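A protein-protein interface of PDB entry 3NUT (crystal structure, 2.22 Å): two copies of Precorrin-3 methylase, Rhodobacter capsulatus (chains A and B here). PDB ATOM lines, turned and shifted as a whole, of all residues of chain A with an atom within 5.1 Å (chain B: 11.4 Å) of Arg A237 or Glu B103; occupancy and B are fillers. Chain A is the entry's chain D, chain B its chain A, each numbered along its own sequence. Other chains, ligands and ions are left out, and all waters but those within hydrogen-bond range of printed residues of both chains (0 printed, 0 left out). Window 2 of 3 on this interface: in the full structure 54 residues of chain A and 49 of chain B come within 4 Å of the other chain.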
ATOM      1  N   LEU A 196     -13.549 -15.844 -33.164  1.00  0.00           N
ATOM      2  CA  LEU A 196     -12.336 -15.337 -32.542  1.00  0.00           C
ATOM      3  C   LEU A 196     -11.189 -15.174 -33.523  1.00  0.00           C
ATOM      4  O   LEU A 196     -10.935 -16.042 -34.362  1.00  0.00           O
ATOM      5  CB  LEU A 196     -11.926 -16.201 -31.343  1.00  0.00           C
ATOM      6  CG  LEU A 196     -12.145 -15.579 -29.963  1.00  0.00           C
ATOM      7  CD1 LEU A 196     -13.389 -14.689 -29.911  1.00  0.00           C
ATOM      8  CD2 LEU A 196     -12.173 -16.676 -28.884  1.00  0.00           C
ATOM      9  N   ALA A 235     -16.707 -22.930 -32.585  1.00  0.00           N
ATOM     10  CA  ALA A 235     -16.738 -23.195 -31.146  1.00  0.00           C
ATOM     11  C   ALA A 235     -15.582 -22.597 -30.321  1.00  0.00           C
ATOM     12  O   ALA A 235     -15.643 -22.623 -29.097  1.00  0.00           O
ATOM     13  CB  ALA A 235     -16.831 -24.677 -30.900  1.00  0.00           C
ATOM     14  N   THR A 236     -14.542 -22.080 -30.981  1.00  0.00           N
ATOM     15  CA  THR A 236     -13.340 -21.548 -30.307  1.00  0.00           C
ATOM     16  C   THR A 236     -13.675 -20.431 -29.324  1.00  0.00           C
ATOM     17  O   THR A 236     -14.315 -19.467 -29.696  1.00  0.00           O
ATOM     18  CB  THR A 236     -12.281 -21.025 -31.334  1.00  0.00           C
ATOM     19  OG1 THR A 236     -11.898 -22.093 -32.213  1.00  0.00           O
ATOM     20  CG2 THR A 236     -11.060 -20.474 -30.626  1.00  0.00           C
ATOM     21  N   ARG A 237     -13.219 -20.563 -28.083  1.00  0.00           N
ATOM     22  CA  ARG A 237     -13.559 -19.622 -27.013  1.00  0.00           C
ATOM     23  C   ARG A 237     -12.372 -19.364 -26.081  1.00  0.00           C
ATOM     24  O   ARG A 237     -11.263 -19.802 -26.366  1.00  0.00           O
ATOM     25  CB  ARG A 237     -14.780 -20.120 -26.226  1.00  0.00           C
ATOM     26  CG  ARG A 237     -14.832 -21.624 -26.043  1.00  0.00           C
ATOM     27  CD  ARG A 237     -15.724 -22.022 -24.901  1.00  0.00           C
ATOM     28  NE  ARG A 237     -15.336 -21.375 -23.647  1.00  0.00           N
ATOM     29  CZ  ARG A 237     -16.011 -21.518 -22.509  1.00  0.00           C
ATOM     30  NH1 ARG A 237     -17.094 -22.287 -22.486  1.00  0.00           N
ATOM     31  NH2 ARG A 237     -15.612 -20.900 -21.401  1.00  0.00           N
ATOM     32  N   ARG A 238     -12.619 -18.646 -24.986  1.00  0.00           N
ATOM     33  CA  ARG A 238     -11.598 -18.266 -24.025  1.00  0.00           C
ATOM     34  C   ARG A 238     -11.723 -18.991 -22.714  1.00  0.00           C
ATOM     35  O   ARG A 238     -12.802 -19.464 -22.352  1.00  0.00           O
ATOM     36  CB  ARG A 238     -11.714 -16.796 -23.671  1.00  0.00           C
ATOM     37  CG  ARG A 238     -11.431 -15.869 -24.804  1.00  0.00           C
ATOM     38  CD  ARG A 238     -11.656 -14.485 -24.332  1.00  0.00           C
ATOM     39  NE  ARG A 238     -12.265 -13.676 -25.380  1.00  0.00           N
ATOM     40  CZ  ARG A 238     -11.609 -12.766 -26.082  1.00  0.00           C
ATOM     41  NH1 ARG A 238     -10.311 -12.563 -25.847  1.00  0.00           N
ATOM     42  NH2 ARG A 238     -12.254 -12.061 -27.004  1.00  0.00           N
ATOM     43  N   VAL A 239     -10.605 -19.029 -21.991  1.00  0.00           N
ATOM     44  CA  VAL A 239     -10.589 -19.384 -20.571  1.00  0.00           C
ATOM     45  C   VAL A 239      -9.387 -18.672 -19.958  1.00  0.00           C
ATOM     46  O   VAL A 239      -8.226 -18.878 -20.374  1.00  0.00           O
ATOM     47  CB  VAL A 239     -10.627 -20.928 -20.308  1.00  0.00           C
ATOM     48  CG1 VAL A 239      -9.544 -21.653 -21.066  1.00  0.00           C
ATOM     49  CG2 VAL A 239     -10.537 -21.236 -18.829  1.00  0.00           C
ATOM     50  N   TRP A 242      -6.348 -17.578 -21.942  1.00  0.00           N
ATOM     51  CA  TRP A 242      -6.046 -18.531 -23.015  1.00  0.00           C
ATOM     52  C   TRP A 242      -7.140 -18.619 -24.059  1.00  0.00           C
ATOM     53  O   TRP A 242      -8.289 -18.296 -23.796  1.00  0.00           O
ATOM     54  CB  TRP A 242      -5.812 -19.945 -22.444  1.00  0.00           C
ATOM     55  CG  TRP A 242      -4.796 -19.988 -21.387  1.00  0.00           C
ATOM     56  CD1 TRP A 242      -5.012 -20.037 -20.044  1.00  0.00           C
ATOM     57  CD2 TRP A 242      -3.385 -20.002 -21.571  1.00  0.00           C
ATOM     58  NE1 TRP A 242      -3.822 -20.071 -19.369  1.00  0.00           N
ATOM     59  CE2 TRP A 242      -2.799 -20.041 -20.278  1.00  0.00           C
ATOM     60  CE3 TRP A 242      -2.556 -19.986 -22.696  1.00  0.00           C
ATOM     61  CZ2 TRP A 242      -1.421 -20.065 -20.075  1.00  0.00           C
ATOM     62  CZ3 TRP A 242      -1.170 -20.014 -22.494  1.00  0.00           C
ATOM     63  CH2 TRP A 242      -0.622 -20.053 -21.194  1.00  0.00           C
ATOM     64  N   VAL A 243      -6.779 -19.118 -25.232  1.00  0.00           N
ATOM     65  CA  VAL A 243      -7.769 -19.475 -26.232  1.00  0.00           C
ATOM     66  C   VAL A 243      -7.659 -20.952 -26.579  1.00  0.00           C
ATOM     67  O   VAL A 243      -6.573 -21.499 -26.681  1.00  0.00           O
ATOM     68  CB  VAL A 243      -7.636 -18.608 -27.477  1.00  0.00           C
ATOM     69  CG1 VAL A 243      -8.721 -18.938 -28.459  1.00  0.00           C
ATOM     70  CG2 VAL A 243      -7.714 -17.151 -27.103  1.00  0.00           C
ATOM     71  N   TYR A 244      -8.797 -21.601 -26.745  1.00  0.00           N
ATOM     72  CA  TYR A 244      -8.814 -23.005 -27.113  1.00  0.00           C
ATOM     73  C   TYR A 244     -10.072 -23.389 -27.880  1.00  0.00           C
ATOM     74  O   TYR A 244     -11.053 -22.646 -27.909  1.00  0.00           O
ATOM     75  CB  TYR A 244      -8.691 -23.890 -25.874  1.00  0.00           C
ATOM     76  CG  TYR A 244      -9.961 -24.020 -25.056  1.00  0.00           C
ATOM     77  CD1 TYR A 244     -10.650 -25.237 -24.981  1.00  0.00           C
ATOM     78  CD2 TYR A 244     -10.453 -22.944 -24.314  1.00  0.00           C
ATOM     79  CE1 TYR A 244     -11.804 -25.375 -24.187  1.00  0.00           C
ATOM     80  CE2 TYR A 244     -11.605 -23.074 -23.524  1.00  0.00           C
ATOM     81  CZ  TYR A 244     -12.278 -24.293 -23.471  1.00  0.00           C
ATOM     82  OH  TYR A 244     -13.417 -24.403 -22.700  1.00  0.00           O
ATOM     83  N   PRO A 246     -12.889 -26.381 -28.106  1.00  0.00           N
ATOM     84  CA  PRO A 246     -13.504 -27.617 -27.544  1.00  0.00           C
ATOM     85  C   PRO A 246     -14.084 -28.596 -28.585  1.00  0.00           C
ATOM     86  O   PRO A 246     -14.398 -29.767 -28.255  1.00  0.00           O
ATOM     87  CB  PRO A 246     -14.631 -27.101 -26.619  1.00  0.00           C
ATOM     88  CG  PRO A 246     -14.784 -25.629 -26.903  1.00  0.00           C
ATOM     89  CD  PRO A 246     -13.759 -25.200 -27.956  1.00  0.00           C
ATOM     90  N   LEU B  65      -9.410 -35.874 -20.136  1.00  0.00           N
ATOM     91  CA  LEU B  65      -9.475 -34.718 -19.253  1.00  0.00           C
ATOM     92  C   LEU B  65      -8.942 -34.962 -17.836  1.00  0.00           C
ATOM     93  O   LEU B  65      -8.381 -34.043 -17.250  1.00  0.00           O
ATOM     94  CB  LEU B  65     -10.886 -34.103 -19.214  1.00  0.00           C
ATOM     95  CG  LEU B  65     -11.515 -33.571 -20.534  1.00  0.00           C
ATOM     96  CD1 LEU B  65     -12.779 -32.720 -20.276  1.00  0.00           C
ATOM     97  CD2 LEU B  65     -10.547 -32.799 -21.460  1.00  0.00           C
ATOM     98  N   ALA B  68      -5.368 -34.332 -17.034  1.00  0.00           N
ATOM     99  CA  ALA B  68      -5.083 -32.900 -17.097  1.00  0.00           C
ATOM    100  C   ALA B  68      -5.488 -32.221 -15.802  1.00  0.00           C
ATOM    101  O   ALA B  68      -4.744 -31.411 -15.283  1.00  0.00           O
ATOM    102  CB  ALA B  68      -5.772 -32.258 -18.293  1.00  0.00           C
ATOM    103  N   THR B  69      -6.657 -32.578 -15.273  1.00  0.00           N
ATOM    104  CA  THR B  69      -7.119 -32.131 -13.961  1.00  0.00           C
ATOM    105  C   THR B  69      -6.109 -32.537 -12.885  1.00  0.00           C
ATOM    106  O   THR B  69      -5.771 -31.758 -11.976  1.00  0.00           O
ATOM    107  CB  THR B  69      -8.540 -32.726 -13.659  1.00  0.00           C
ATOM    108  OG1 THR B  69      -9.450 -32.363 -14.721  1.00  0.00           O
ATOM    109  CG2 THR B  69      -9.089 -32.253 -12.318  1.00  0.00           C
ATOM    110  N   LEU B  72      -3.122 -30.379 -13.041  1.00  0.00           N
ATOM    111  CA  LEU B  72      -3.412 -29.095 -12.410  1.00  0.00           C
ATOM    112  C   LEU B  72      -3.339 -29.193 -10.897  1.00  0.00           C
ATOM    113  O   LEU B  72      -2.867 -28.262 -10.239  1.00  0.00           O
ATOM    114  CB  LEU B  72      -4.784 -28.561 -12.824  1.00  0.00           C
ATOM    115  CG  LEU B  72      -5.089 -28.160 -14.262  1.00  0.00           C
ATOM    116  CD1 LEU B  72      -6.570 -27.849 -14.319  1.00  0.00           C
ATOM    117  CD2 LEU B  72      -4.274 -26.931 -14.670  1.00  0.00           C
ATOM    118  N   MET B  94      -2.800 -32.958 -26.229  1.00  0.00           N
ATOM    119  CA  MET B  94      -3.132 -32.680 -24.838  1.00  0.00           C
ATOM    120  C   MET B  94      -3.325 -31.187 -24.447  1.00  0.00           C
ATOM    121  O   MET B  94      -3.921 -30.890 -23.400  1.00  0.00           O
ATOM    122  CB  MET B  94      -2.107 -33.362 -23.916  1.00  0.00           C
ATOM    123  CG  MET B  94      -2.390 -34.839 -23.624  1.00  0.00           C
ATOM    124  SD  MET B  94      -3.971 -35.113 -22.764  1.00  0.00           S
ATOM    125  CE  MET B  94      -3.731 -34.201 -21.251  1.00  0.00           C
ATOM    126  N   ALA B  95      -2.826 -30.262 -25.259  1.00  0.00           N
ATOM    127  CA  ALA B  95      -2.955 -28.846 -24.924  1.00  0.00           C
ATOM    128  C   ALA B  95      -4.429 -28.424 -24.818  1.00  0.00           C
ATOM    129  O   ALA B  95      -4.818 -27.782 -23.828  1.00  0.00           O
ATOM    130  CB  ALA B  95      -2.181 -27.961 -25.886  1.00  0.00           C
ATOM    131  N   SER B  96      -5.229 -28.804 -25.821  1.00  0.00           N
ATOM    132  CA  SER B  96      -6.691 -28.630 -25.814  1.00  0.00           C
ATOM    133  C   SER B  96      -7.407 -29.149 -24.560  1.00  0.00           C
ATOM    134  O   SER B  96      -8.207 -28.436 -23.943  1.00  0.00           O
ATOM    135  CB  SER B  96      -7.305 -29.364 -27.007  1.00  0.00           C
ATOM    136  OG  SER B  96      -7.788 -28.436 -27.948  1.00  0.00           O
ATOM    137  N   ALA B  97      -7.134 -30.408 -24.240  1.00  0.00           N
ATOM    138  CA  ALA B  97      -7.684 -31.075 -23.087  1.00  0.00           C
ATOM    139  C   ALA B  97      -7.308 -30.394 -21.779  1.00  0.00           C
ATOM    140  O   ALA B  97      -8.098 -30.372 -20.850  1.00  0.00           O
ATOM    141  CB  ALA B  97      -7.198 -32.502 -23.055  1.00  0.00           C
ATOM    142  N   LEU B  98      -6.090 -29.870 -21.695  1.00  0.00           N
ATOM    143  CA  LEU B  98      -5.689 -29.137 -20.494  1.00  0.00           C
ATOM    144  C   LEU B  98      -6.558 -27.894 -20.311  1.00  0.00           C
ATOM    145  O   LEU B  98      -6.987 -27.596 -19.185  1.00  0.00           O
ATOM    146  CB  LEU B  98      -4.191 -28.775 -20.506  1.00  0.00           C
ATOM    147  CG  LEU B  98      -3.685 -27.822 -19.403  1.00  0.00           C
ATOM    148  CD1 LEU B  98      -3.822 -28.476 -18.025  1.00  0.00           C
ATOM    149  CD2 LEU B  98      -2.232 -27.380 -19.651  1.00  0.00           C
ATOM    150  N   PHE B  99      -6.820 -27.188 -21.403  1.00  0.00           N
ATOM    151  CA  PHE B  99      -7.635 -25.982 -21.341  1.00  0.00           C
ATOM    152  C   PHE B  99      -9.105 -26.327 -21.129  1.00  0.00           C
ATOM    153  O   PHE B  99      -9.823 -25.584 -20.432  1.00  0.00           O
ATOM    154  CB  PHE B  99      -7.401 -25.056 -22.536  1.00  0.00           C
ATOM    155  CG  PHE B  99      -6.000 -24.541 -22.593  1.00  0.00           C
ATOM    156  CD1 PHE B  99      -5.515 -23.728 -21.586  1.00  0.00           C
ATOM    157  CD2 PHE B  99      -5.137 -24.918 -23.621  1.00  0.00           C
ATOM    158  CE1 PHE B  99      -4.208 -23.274 -21.616  1.00  0.00           C
ATOM    159  CE2 PHE B  99      -3.843 -24.468 -23.650  1.00  0.00           C
ATOM    160  CZ  PHE B  99      -3.364 -23.663 -22.662  1.00  0.00           C
ATOM    161  N   GLU B 100      -9.532 -27.471 -21.666  1.00  0.00           N
ATOM    162  CA  GLU B 100     -10.821 -28.041 -21.241  1.00  0.00           C
ATOM    163  C   GLU B 100     -10.912 -28.400 -19.747  1.00  0.00           C
ATOM    164  O   GLU B 100     -11.907 -28.067 -19.118  1.00  0.00           O
ATOM    165  CB  GLU B 100     -11.253 -29.229 -22.095  1.00  0.00           C
ATOM    166  CG  GLU B 100     -11.731 -28.821 -23.455  1.00  0.00           C
ATOM    167  CD  GLU B 100     -11.930 -30.009 -24.403  1.00  0.00           C
ATOM    168  OE1 GLU B 100     -11.090 -30.170 -25.320  1.00  0.00           O
ATOM    169  OE2 GLU B 100     -12.933 -30.752 -24.226  1.00  0.00           O
ATOM    170  N   ALA B 101      -9.911 -29.070 -19.186  1.00  0.00           N
ATOM    171  CA  ALA B 101      -9.943 -29.352 -17.759  1.00  0.00           C
ATOM    172  C   ALA B 101      -9.905 -28.068 -16.920  1.00  0.00           C
ATOM    173  O   ALA B 101     -10.556 -27.987 -15.912  1.00  0.00           O
ATOM    174  CB  ALA B 101      -8.811 -30.276 -17.362  1.00  0.00           C
ATOM    175  N   LEU B 102      -9.131 -27.073 -17.356  1.00  0.00           N
ATOM    176  CA  LEU B 102      -9.107 -25.776 -16.720  1.00  0.00           C
ATOM    177  C   LEU B 102     -10.466 -25.038 -16.730  1.00  0.00           C
ATOM    178  O   LEU B 102     -10.933 -24.558 -15.690  1.00  0.00           O
ATOM    179  CB  LEU B 102      -7.984 -24.910 -17.315  1.00  0.00           C
ATOM    180  CG  LEU B 102      -7.904 -23.476 -16.771  1.00  0.00           C
ATOM    181  CD1 LEU B 102      -7.395 -23.462 -15.325  1.00  0.00           C
ATOM    182  CD2 LEU B 102      -7.066 -22.569 -17.685  1.00  0.00           C
ATOM    183  N   GLU B 103     -11.107 -24.954 -17.881  1.00  0.00           N
ATOM    184  CA  GLU B 103     -12.429 -24.362 -17.958  1.00  0.00           C
ATOM    185  C   GLU B 103     -13.431 -25.090 -17.030  1.00  0.00           C
ATOM    186  O   GLU B 103     -14.315 -24.452 -16.446  1.00  0.00           O
ATOM    187  CB  GLU B 103     -12.925 -24.330 -19.406  1.00  0.00           C
ATOM    188  CG  GLU B 103     -14.142 -23.440 -19.657  1.00  0.00           C
ATOM    189  CD  GLU B 103     -15.490 -24.164 -19.428  1.00  0.00           C
ATOM    190  OE1 GLU B 103     -16.525 -23.460 -19.243  1.00  0.00           O
ATOM    191  OE2 GLU B 103     -15.524 -25.429 -19.419  1.00  0.00           O
ATOM    192  N   ALA B 104     -13.282 -26.405 -16.874  1.00  0.00           N
ATOM    193  CA  ALA B 104     -14.222 -27.159 -16.036  1.00  0.00           C
ATOM    194  C   ALA B 104     -13.889 -27.073 -14.558  1.00  0.00           C
ATOM    195  O   ALA B 104     -14.689 -27.505 -13.712  1.00  0.00           O
ATOM    196  CB  ALA B 104     -14.286 -28.613 -16.457  1.00  0.00           C
ATOM    197  N   HIS B 105     -12.724 -26.529 -14.230  1.00  0.00           N
ATOM    198  CA  HIS B 105     -12.328 -26.440 -12.817  1.00  0.00           C
ATOM    199  C   HIS B 105     -11.839 -25.038 -12.474  1.00  0.00           C
ATOM    200  O   HIS B 105     -10.629 -24.793 -12.409  1.00  0.00           O
ATOM    201  CB  HIS B 105     -11.260 -27.478 -12.493  1.00  0.00           C
ATOM    202  CG  HIS B 105     -11.716 -28.882 -12.697  1.00  0.00           C
ATOM    203  ND1 HIS B 105     -11.816 -29.462 -13.952  1.00  0.00           N
ATOM    204  CD2 HIS B 105     -12.099 -29.832 -11.811  1.00  0.00           C
ATOM    205  CE1 HIS B 105     -12.246 -30.703 -13.825  1.00  0.00           C
ATOM    206  NE2 HIS B 105     -12.420 -30.954 -12.539  1.00  0.00           N
ATOM    207  N   PRO B 106     -12.776 -24.106 -12.246  1.00  0.00           N
ATOM    208  CA  PRO B 106     -12.359 -22.740 -11.908  1.00  0.00           C
ATOM    209  C   PRO B 106     -11.457 -22.619 -10.648  1.00  0.00           C
ATOM    210  O   PRO B 106     -10.784 -21.604 -10.464  1.00  0.00           O
ATOM    211  CB  PRO B 106     -13.698 -21.983 -11.746  1.00  0.00           C
ATOM    212  CG  PRO B 106     -14.758 -23.037 -11.616  1.00  0.00           C
ATOM    213  CD  PRO B 106     -14.249 -24.220 -12.383  1.00  0.00           C
ATOM    214  N   GLU B 107     -11.393 -23.661  -9.828  1.00  0.00           N
ATOM    215  CA  GLU B 107     -10.523 -23.628  -8.636  1.00  0.00           C
ATOM    216  C   GLU B 107      -8.993 -23.604  -8.925  1.00  0.00           C
ATOM    217  O   GLU B 107      -8.178 -23.382  -8.012  1.00  0.00           O
ATOM    218  CB  GLU B 107     -10.943 -24.690  -7.576  1.00  0.00           C
ATOM    219  CG  GLU B 107     -10.805 -26.210  -7.924  1.00  0.00           C
ATOM    220  CD  GLU B 107     -11.838 -26.774  -8.947  1.00  0.00           C
ATOM    221  OE1 GLU B 107     -12.699 -26.019  -9.470  1.00  0.00           O
ATOM    222  OE2 GLU B 107     -11.793 -28.005  -9.223  1.00  0.00           O
ATOM    223  N   HIS B 108      -8.639 -23.820 -10.206  1.00  0.00           N
ATOM    224  CA  HIS B 108      -7.259 -23.904 -10.698  1.00  0.00           C
ATOM    225  C   HIS B 108      -6.998 -22.737 -11.661  1.00  0.00           C
ATOM    226  O   HIS B 108      -5.962 -22.665 -12.324  1.00  0.00           O
ATOM    227  CB  HIS B 108      -7.016 -25.269 -11.411  1.00  0.00           C
ATOM    228  CG  HIS B 108      -7.228 -26.466 -10.529  1.00  0.00           C
ATOM    229  ND1 HIS B 108      -6.652 -26.582  -9.283  1.00  0.00           N
ATOM    230  CD2 HIS B 108      -7.959 -27.597 -10.706  1.00  0.00           C
ATOM    231  CE1 HIS B 108      -7.023 -27.719  -8.721  1.00  0.00           C
ATOM    232  NE2 HIS B 108      -7.818 -28.354  -9.562  1.00  0.00           N
ATOM    233  N   ALA B 109      -7.977 -21.840 -11.774  1.00  0.00           N
ATOM    234  CA  ALA B 109      -7.790 -20.586 -12.475  1.00  0.00           C
ATOM    235  C   ALA B 109      -6.538 -19.932 -11.880  1.00  0.00           C
ATOM    236  O   ALA B 109      -6.371 -19.894 -10.649  1.00  0.00           O
ATOM    237  CB  ALA B 109      -9.010 -19.680 -12.267  1.00  0.00           C
ATOM    238  N   GLY B 110      -5.666 -19.431 -12.749  1.00  0.00           N
ATOM    239  CA  GLY B 110      -4.413 -18.855 -12.278  1.00  0.00           C
ATOM    240  C   GLY B 110      -3.207 -19.789 -12.312  1.00  0.00           C
ATOM    241  O   GLY B 110      -2.080 -19.309 -12.279  1.00  0.00           O
ATOM    242  N   THR B 111      -3.418 -21.106 -12.392  1.00  0.00           N
ATOM    243  CA  THR B 111      -2.293 -22.030 -12.556  1.00  0.00           C
ATOM    244  C   THR B 111      -1.353 -21.535 -13.660  1.00  0.00           C
ATOM    245  O   THR B 111      -1.814 -21.099 -14.707  1.00  0.00           O
ATOM    246  CB  THR B 111      -2.750 -23.506 -12.896  1.00  0.00           C
ATOM    247  OG1 THR B 111      -3.724 -23.988 -11.945  1.00  0.00           O
ATOM    248  CG2 THR B 111      -1.544 -24.471 -12.917  1.00  0.00           C
ATOM    249  N   ILE B 113       0.781 -22.054 -16.833  1.00  0.00           N
ATOM    250  CA  ILE B 113       0.667 -23.034 -17.881  1.00  0.00           C
ATOM    251  C   ILE B 113       1.551 -22.607 -19.031  1.00  0.00           C
ATOM    252  O   ILE B 113       1.570 -21.450 -19.371  1.00  0.00           O
ATOM    253  CB  ILE B 113      -0.789 -23.204 -18.387  1.00  0.00           C
ATOM    254  CG1 ILE B 113      -1.551 -24.154 -17.462  1.00  0.00           C
ATOM    255  CG2 ILE B 113      -0.785 -23.820 -19.781  1.00  0.00           C
ATOM    256  CD1 ILE B 113      -3.093 -23.887 -17.362  1.00  0.00           C
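The side-chain carboxylate (OE1) of Glu B103 is in salt-bridge range of the guanidinium group (NH2) of Arg A237, 3.5 Å away.
Val A239 touches Phe B99. Leu B102 touches Val A239 (CD2 to CG2, 3.9 Å). Glu B103 touches Val A239. Trp A242 touches Phe B99. CH2 of Trp A242 touches O of Ile B113, 3.2 Å away. CG of Tyr A244 touches CB of Phe B99 (3.7 Å). Glu B100 touches Tyr A244 (CG to CE1, 3.5 Å). Glu B103 touches Tyr A244 (CG to OH, 3.3 Å).
Arg A237 touches just one residue of chain B: Glu B103. Glu B103 touches just these residues of chain A: Arg A237 (3.4 Å), Val A239 (3.8 Å) and Tyr A244 (3.3 Å). No residue of chain B comes within 4 Å of Thr A236. No residue of chain B comes within 4 Å of Val A243. Of chain B, only Phe B99 (3.7 Å), Glu B100 (3.5 Å) and Glu B103 (3.3 Å) come within 4 Å of Tyr A244. Printed residues of chain A within 4 Å of Ile B113: Trp A242. Of the printed residues of chain B, Val A239 touches Phe B99, Leu B102 and Glu B103. Of the printed residues of chain A, Leu B102 touches Val A239 (3.9 Å). Of the printed residues of chain A, Phe B99 touches Val A239 (3.99 Å), Trp A242 (3.3 Å) and Tyr A244 (3.7 Å). Of the printed residues of chain A, Glu B100 touches Tyr A244 (3.5 Å).
Printed residues of chain A that touch a printed residue of chain B: Arg A237, Val A239, Trp A242 and Tyr A244. Hydrophobic or aromatic side chains of chain A within 4 Å of the printed part of chain B: Val A239, Trp A242 and Tyr A244. Among the printed residues, Asp or Glu carboxylates within 4 Å of a Lys or Arg side-chain nitrogen of the other chain: Arg A237 with Glu B103 (3.5 Å).
The backbone carbonyl oxygen (O) of Tyr A244 sits at hydrogen-bond distance from the backbone NH (N) of Arg A237.
No position is printed for both chains.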
